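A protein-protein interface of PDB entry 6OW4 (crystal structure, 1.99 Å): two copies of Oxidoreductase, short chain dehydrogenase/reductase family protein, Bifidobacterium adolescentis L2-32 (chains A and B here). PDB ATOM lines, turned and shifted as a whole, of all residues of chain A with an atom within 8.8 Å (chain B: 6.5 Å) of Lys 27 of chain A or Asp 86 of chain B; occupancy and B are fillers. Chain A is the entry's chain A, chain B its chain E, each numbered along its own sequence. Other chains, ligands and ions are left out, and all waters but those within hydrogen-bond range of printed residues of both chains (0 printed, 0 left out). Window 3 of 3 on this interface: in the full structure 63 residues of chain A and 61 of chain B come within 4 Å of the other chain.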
ATOM      1  N   LEU A  23     -22.304  16.609  15.396  1.00  0.00           N
ATOM      2  CA  LEU A  23     -21.822  16.047  14.105  1.00  0.00           C
ATOM      3  C   LEU A  23     -21.954  14.519  14.108  1.00  0.00           C
ATOM      4  O   LEU A  23     -22.279  13.964  13.038  1.00  0.00           O
ATOM      5  CB  LEU A  23     -20.369  16.479  13.869  1.00  0.00           C
ATOM      6  CG  LEU A  23     -20.190  17.791  13.106  1.00  0.00           C
ATOM      7  CD1 LEU A  23     -20.799  18.957  13.863  1.00  0.00           C
ATOM      8  CD2 LEU A  23     -18.721  18.052  12.823  1.00  0.00           C
ATOM      9  N   ASP A  24     -21.708  13.868  15.251  1.00  0.00           N
ATOM     10  CA  ASP A  24     -21.634  12.385  15.363  1.00  0.00           C
ATOM     11  C   ASP A  24     -22.274  11.919  16.677  1.00  0.00           C
ATOM     12  O   ASP A  24     -21.525  11.613  17.625  1.00  0.00           O
ATOM     13  CB  ASP A  24     -20.184  11.904  15.244  1.00  0.00           C
ATOM     14  CG  ASP A  24     -19.494  12.360  13.970  1.00  0.00           C
ATOM     15  OD1 ASP A  24     -18.955  13.484  13.965  1.00  0.00           O
ATOM     16  OD2 ASP A  24     -19.515  11.597  12.987  1.00  0.00           O
ATOM     17  N   LYS A  25     -23.608  11.837  16.710  1.00  0.00           N
ATOM     18  CA  LYS A  25     -24.397  11.356  17.881  1.00  0.00           C
ATOM     19  C   LYS A  25     -24.128   9.864  18.120  1.00  0.00           C
ATOM     20  O   LYS A  25     -24.192   9.440  19.292  1.00  0.00           O
ATOM     21  CB  LYS A  25     -25.892  11.603  17.666  1.00  0.00           C
ATOM     22  CG  LYS A  25     -26.310  13.065  17.667  1.00  0.00           C
ATOM     23  CD  LYS A  25     -27.809  13.261  17.628  1.00  0.00           C
ATOM     24  CE  LYS A  25     -28.205  14.705  17.406  1.00  0.00           C
ATOM     25  NZ  LYS A  25     -29.677  14.877  17.385  1.00  0.00           N
ATOM     26  N   TRP A  26     -23.840   9.106  17.055  1.00  0.00           N
ATOM     27  CA  TRP A  26     -23.546   7.644  17.100  1.00  0.00           C
ATOM     28  C   TRP A  26     -22.341   7.351  18.006  1.00  0.00           C
ATOM     29  O   TRP A  26     -22.221   6.193  18.458  1.00  0.00           O
ATOM     30  CB  TRP A  26     -23.337   7.078  15.688  1.00  0.00           C
ATOM     31  CG  TRP A  26     -22.194   7.682  14.929  1.00  0.00           C
ATOM     32  CD1 TRP A  26     -22.235   8.790  14.137  1.00  0.00           C
ATOM     33  CD2 TRP A  26     -20.841   7.195  14.866  1.00  0.00           C
ATOM     34  NE1 TRP A  26     -21.003   9.039  13.597  1.00  0.00           N
ATOM     35  CE2 TRP A  26     -20.126   8.077  14.025  1.00  0.00           C
ATOM     36  CE3 TRP A  26     -20.163   6.111  15.435  1.00  0.00           C
ATOM     37  CZ2 TRP A  26     -18.773   7.904  13.744  1.00  0.00           C
ATOM     38  CZ3 TRP A  26     -18.824   5.941  15.157  1.00  0.00           C
ATOM     39  CH2 TRP A  26     -18.141   6.826  14.323  1.00  0.00           C
ATOM     40  N   LYS A  27     -21.481   8.346  18.258  1.00  0.00           N
ATOM     41  CA  LYS A  27     -20.295   8.215  19.151  1.00  0.00           C
ATOM     42  C   LYS A  27     -20.739   8.127  20.620  1.00  0.00           C
ATOM     43  O   LYS A  27     -19.907   7.717  21.450  1.00  0.00           O
ATOM     44  CB  LYS A  27     -19.314   9.372  18.925  1.00  0.00           C
ATOM     45  CG  LYS A  27     -18.508   9.286  17.633  1.00  0.00           C
ATOM     46  CD  LYS A  27     -17.007   9.359  17.838  1.00  0.00           C
ATOM     47  CE  LYS A  27     -16.473   8.202  18.659  1.00  0.00           C
ATOM     48  NZ  LYS A  27     -14.992   8.130  18.639  1.00  0.00           N
ATOM     49  N   ASP A  28     -21.986   8.507  20.930  1.00  0.00           N
ATOM     50  CA  ASP A  28     -22.644   8.266  22.243  1.00  0.00           C
ATOM     51  C   ASP A  28     -23.175   6.827  22.260  1.00  0.00           C
ATOM     52  O   ASP A  28     -24.040   6.512  21.422  1.00  0.00           O
ATOM     53  CB  ASP A  28     -23.764   9.281  22.497  1.00  0.00           C
ATOM     54  CG  ASP A  28     -24.480   9.117  23.828  1.00  0.00           C
ATOM     55  OD1 ASP A  28     -24.043   8.277  24.639  1.00  0.00           O
ATOM     56  OD2 ASP A  28     -25.476   9.836  24.041  1.00  0.00           O
ATOM     57  N   SER A  29     -22.685   5.998  23.187  1.00  0.00           N
ATOM     58  CA  SER A  29     -22.984   4.543  23.279  1.00  0.00           C
ATOM     59  C   SER A  29     -24.440   4.313  23.709  1.00  0.00           C
ATOM     60  O   SER A  29     -24.984   3.243  23.370  1.00  0.00           O
ATOM     61  CB  SER A  29     -22.024   3.847  24.212  1.00  0.00           C
ATOM     62  OG  SER A  29     -22.309   4.161  25.567  1.00  0.00           O
ATOM     63  N   ASN A  30     -25.041   5.272  24.424  1.00  0.00           N
ATOM     64  CA  ASN A  30     -26.433   5.187  24.946  1.00  0.00           C
ATOM     65  C   ASN A  30     -27.427   5.734  23.913  1.00  0.00           C
ATOM     66  O   ASN A  30     -28.642   5.678  24.191  1.00  0.00           O
ATOM     67  CB  ASN A  30     -26.578   5.916  26.285  1.00  0.00           C
ATOM     68  CG  ASN A  30     -25.721   5.314  27.377  1.00  0.00           C
ATOM     69  OD1 ASN A  30     -25.002   6.028  28.073  1.00  0.00           O
ATOM     70  ND2 ASN A  30     -25.780   4.000  27.529  1.00  0.00           N
ATOM     71  N   TYR A  31     -26.940   6.242  22.776  1.00  0.00           N
ATOM     72  CA  TYR A  31     -27.764   6.693  21.621  1.00  0.00           C
ATOM     73  C   TYR A  31     -27.935   5.524  20.643  1.00  0.00           C
ATOM     74  O   TYR A  31     -27.019   4.682  20.546  1.00  0.00           O
ATOM     75  CB  TYR A  31     -27.126   7.911  20.944  1.00  0.00           C
ATOM     76  CG  TYR A  31     -27.666   8.248  19.576  1.00  0.00           C
ATOM     77  CD1 TYR A  31     -28.775   9.065  19.423  1.00  0.00           C
ATOM     78  CD2 TYR A  31     -27.060   7.760  18.430  1.00  0.00           C
ATOM     79  CE1 TYR A  31     -29.269   9.385  18.168  1.00  0.00           C
ATOM     80  CE2 TYR A  31     -27.542   8.069  17.168  1.00  0.00           C
ATOM     81  CZ  TYR A  31     -28.652   8.885  17.036  1.00  0.00           C
ATOM     82  OH  TYR A  31     -29.133   9.196  15.797  1.00  0.00           O
ATOM     83  N   SER A  32     -29.081   5.474  19.958  1.00  0.00           N
ATOM     84  CA  SER A  32     -29.371   4.523  18.852  1.00  0.00           C
ATOM     85  C   SER A  32     -30.320   5.172  17.841  1.00  0.00           C
ATOM     86  O   SER A  32     -31.380   5.681  18.258  1.00  0.00           O
ATOM     87  CB  SER A  32     -29.932   3.224  19.365  1.00  0.00           C
ATOM     88  OG  SER A  32     -30.155   2.319  18.292  1.00  0.00           O
ATOM     89  N   THR B  81     -10.217   4.427   7.909  1.00  0.00           N
ATOM     90  CA  THR B  81      -9.696   3.287   8.713  1.00  0.00           C
ATOM     91  C   THR B  81     -10.132   3.457  10.174  1.00  0.00           C
ATOM     92  O   THR B  81     -10.692   2.495  10.734  1.00  0.00           O
ATOM     93  CB  THR B  81      -8.172   3.163   8.598  1.00  0.00           C
ATOM     94  OG1 THR B  81      -7.821   3.256   7.216  1.00  0.00           O
ATOM     95  CG2 THR B  81      -7.640   1.868   9.173  1.00  0.00           C
ATOM     96  N   GLU B  82      -9.891   4.640  10.753  1.00  0.00           N
ATOM     97  CA  GLU B  82     -10.244   4.986  12.158  1.00  0.00           C
ATOM     98  C   GLU B  82     -11.757   4.826  12.362  1.00  0.00           C
ATOM     99  O   GLU B  82     -12.150   4.149  13.331  1.00  0.00           O
ATOM    100  CB  GLU B  82      -9.794   6.409  12.491  1.00  0.00           C
ATOM    101  CG  GLU B  82      -8.288   6.554  12.631  1.00  0.00           C
ATOM    102  CD  GLU B  82      -7.787   7.985  12.758  1.00  0.00           C
ATOM    103  OE1 GLU B  82      -8.629   8.908  12.769  1.00  0.00           O
ATOM    104  OE2 GLU B  82      -6.555   8.173  12.847  1.00  0.00           O
ATOM    105  N   LEU B  83     -12.563   5.422  11.476  1.00  0.00           N
ATOM    106  CA  LEU B  83     -14.052   5.377  11.517  1.00  0.00           C
ATOM    107  C   LEU B  83     -14.542   3.931  11.357  1.00  0.00           C
ATOM    108  O   LEU B  83     -15.487   3.550  12.074  1.00  0.00           O
ATOM    109  CB  LEU B  83     -14.623   6.269  10.407  1.00  0.00           C
ATOM    110  CG  LEU B  83     -14.530   7.776  10.646  1.00  0.00           C
ATOM    111  CD1 LEU B  83     -14.808   8.545   9.362  1.00  0.00           C
ATOM    112  CD2 LEU B  83     -15.486   8.216  11.744  1.00  0.00           C
ATOM    113  N   ALA B  84     -13.930   3.167  10.445  1.00  0.00           N
ATOM    114  CA  ALA B  84     -14.293   1.764  10.126  1.00  0.00           C
ATOM    115  C   ALA B  84     -14.009   0.863  11.335  1.00  0.00           C
ATOM    116  O   ALA B  84     -14.833  -0.030  11.608  1.00  0.00           O
ATOM    117  CB  ALA B  84     -13.542   1.295   8.903  1.00  0.00           C
ATOM    118  N   LYS B  85     -12.880   1.084  12.017  1.00  0.00           N
ATOM    119  CA  LYS B  85     -12.480   0.332  13.238  1.00  0.00           C
ATOM    120  C   LYS B  85     -13.401   0.730  14.397  1.00  0.00           C
ATOM    121  O   LYS B  85     -13.749  -0.156  15.204  1.00  0.00           O
ATOM    122  CB  LYS B  85     -11.012   0.598  13.584  1.00  0.00           C
ATOM    123  CG  LYS B  85      -9.999  -0.016  12.626  1.00  0.00           C
ATOM    124  CD  LYS B  85      -8.562   0.031  13.113  1.00  0.00           C
ATOM    125  CE  LYS B  85      -8.191   1.325  13.808  1.00  0.00           C
ATOM    126  NZ  LYS B  85      -6.747   1.374  14.139  1.00  0.00           N
ATOM    127  N   ASP B  86     -13.783   2.011  14.462  1.00  0.00           N
ATOM    128  CA  ASP B  86     -14.670   2.585  15.508  1.00  0.00           C
ATOM    129  C   ASP B  86     -16.058   1.935  15.411  1.00  0.00           C
ATOM    130  O   ASP B  86     -16.513   1.373  16.425  1.00  0.00           O
ATOM    131  CB  ASP B  86     -14.745   4.113  15.388  1.00  0.00           C
ATOM    132  CG  ASP B  86     -15.386   4.814  16.575  1.00  0.00           C
ATOM    133  OD1 ASP B  86     -15.835   4.116  17.507  1.00  0.00           O
ATOM    134  OD2 ASP B  86     -15.430   6.061  16.558  1.00  0.00           O
ATOM    135  N   MET B  87     -16.691   2.000  14.233  1.00  0.00           N
ATOM    136  CA  MET B  87     -18.081   1.520  13.991  1.00  0.00           C
ATOM    137  C   MET B  87     -18.160  -0.003  14.166  1.00  0.00           C
ATOM    138  O   MET B  87     -19.220  -0.484  14.614  1.00  0.00           O
ATOM    139  CB  MET B  87     -18.559   1.895  12.584  1.00  0.00           C
ATOM    140  CG  MET B  87     -18.801   3.383  12.406  1.00  0.00           C
ATOM    141  SD  MET B  87     -19.353   3.809  10.734  1.00  0.00           S
ATOM    142  CE  MET B  87     -18.984   5.562  10.701  1.00  0.00           C
ATOM    143  N   SER B  88     -17.094  -0.733  13.824  1.00  0.00           N
ATOM    144  CA  SER B  88     -17.007  -2.213  13.947  1.00  0.00           C
ATOM    145  C   SER B  88     -17.113  -2.623  15.422  1.00  0.00           C
ATOM    146  O   SER B  88     -17.925  -3.519  15.723  1.00  0.00           O
ATOM    147  CB  SER B  88     -15.743  -2.742  13.320  1.00  0.00           C
ATOM    148  OG  SER B  88     -15.750  -2.534  11.916  1.00  0.00           O
ATOM    149  N   GLU B  89     -16.324  -1.986  16.296  1.00  0.00           N
ATOM    150  CA  GLU B  89     -16.325  -2.219  17.768  1.00  0.00           C
ATOM    151  C   GLU B  89     -17.704  -1.892  18.350  1.00  0.00           C
ATOM    152  O   GLU B  89     -18.165  -2.654  19.221  1.00  0.00           O
ATOM    153  CB  GLU B  89     -15.273  -1.359  18.473  1.00  0.00           C
ATOM    154  CG  GLU B  89     -13.892  -1.986  18.515  1.00  0.00           C
ATOM    155  CD  GLU B  89     -12.912  -1.263  19.425  1.00  0.00           C
ATOM    156  OE1 GLU B  89     -12.890  -0.013  19.393  1.00  0.00           O
ATOM    157  OE2 GLU B  89     -12.176  -1.946  20.171  1.00  0.00           O
ATOM    158  N   ARG B  90     -18.322  -0.799  17.890  1.00  0.00           N
ATOM    159  CA  ARG B  90     -19.573  -0.228  18.461  1.00  0.00           C
ATOM    160  C   ARG B  90     -20.770  -1.128  18.141  1.00  0.00           C
ATOM    161  O   ARG B  90     -21.492  -1.496  19.084  1.00  0.00           O
ATOM    162  CB  ARG B  90     -19.814   1.190  17.933  1.00  0.00           C
ATOM    163  CG  ARG B  90     -18.982   2.246  18.642  1.00  0.00           C
ATOM    164  CD  ARG B  90     -19.260   3.657  18.171  1.00  0.00           C
ATOM    165  NE  ARG B  90     -18.406   4.591  18.893  1.00  0.00           N
ATOM    166  CZ  ARG B  90     -18.675   5.116  20.087  1.00  0.00           C
ATOM    167  NH1 ARG B  90     -19.805   4.830  20.715  1.00  0.00           N
ATOM    168  NH2 ARG B  90     -17.812   5.946  20.646  1.00  0.00           N
ATOM    169  N   PHE B  91     -20.975  -1.456  16.863  1.00  0.00           N
ATOM    170  CA  PHE B  91     -22.220  -2.081  16.341  1.00  0.00           C
ATOM    171  C   PHE B  91     -22.005  -3.571  16.044  1.00  0.00           C
ATOM    172  O   PHE B  91     -22.988  -4.239  15.672  1.00  0.00           O
ATOM    173  CB  PHE B  91     -22.706  -1.296  15.121  1.00  0.00           C
ATOM    174  CG  PHE B  91     -22.780   0.194  15.350  1.00  0.00           C
ATOM    175  CD1 PHE B  91     -23.429   0.706  16.466  1.00  0.00           C
ATOM    176  CD2 PHE B  91     -22.191   1.085  14.465  1.00  0.00           C
ATOM    177  CE1 PHE B  91     -23.493   2.073  16.685  1.00  0.00           C
ATOM    178  CE2 PHE B  91     -22.257   2.452  14.685  1.00  0.00           C
ATOM    179  CZ  PHE B  91     -22.909   2.943  15.795  1.00  0.00           C
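The side-chain amino group (NZ) of Lys 27 of chain A is in salt-bridge range of the side-chain carboxylate (OD2) of Asp 86 of chain B, at 3.0 Å. NH2 of Arg 90 of chain B lies within hydrogen-bond range of O of Lys 27 of chain A, at 2.9 Å.
The indole nitrogen (NE1) of Trp 26 of chain A lies within hydrogen-bond range of the side-chain carboxylate (OD2) of Asp 24 of chain A. The guanidinium group of Arg 90 of chain B is in salt-bridge range of the side-chain carboxylate of Asp 86 of chain B.
Leu 83 of chain B touches Trp 26 of chain A. Trp 26 of chain A touches Asp 86 of chain B. Trp 26 of chain A touches Met 87 of chain B (CZ3 to CG, 3.8 Å). Arg 90 of chain B touches Trp 26 of chain A. NH1 of Arg 90 of chain B touches N of Ser 29 of chain A (3.97 Å).
Of chain B, only Asp 86 and Arg 90 come within 4 Å of Lys 27 of chain A. Asp 86 of chain B touches just these residues of chain A: Trp 26 (3.6 Å) and Lys 27 (3.0 Å). Of the printed residues of chain A, Arg 90 of chain B touches Trp 26 (3.6 Å), Lys 27 (2.9 Å) and Ser 29 (3.97 Å). Printed residues of chain A within 4 Å of Met 87 of chain B: Trp 26. Of the printed residues of chain A, Leu 83 of chain B touches Trp 26 (3.9 Å). Printed residues of chain B within 4 Å of Ser 29 of chain A: Arg 90 (3.97 Å). Of the printed residues of chain B, Trp 26 of chain A touches Leu 83, Asp 86, Met 87 and Arg 90. The nearest residue of chain B that does not touch Lys 27 of chain A is Phe 91 of chain B (6.1 Å). The nearest residue of chain A that does not touch Asp 86 of chain B is Asp 24 of chain A (7.6 Å).
Among the printed residues, Asp or Glu carboxylates within 4 Å of a Lys or Arg side-chain nitrogen of the other chain: Lys 27 of chain A with Asp 86 of chain B.
No position is printed for both chains.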
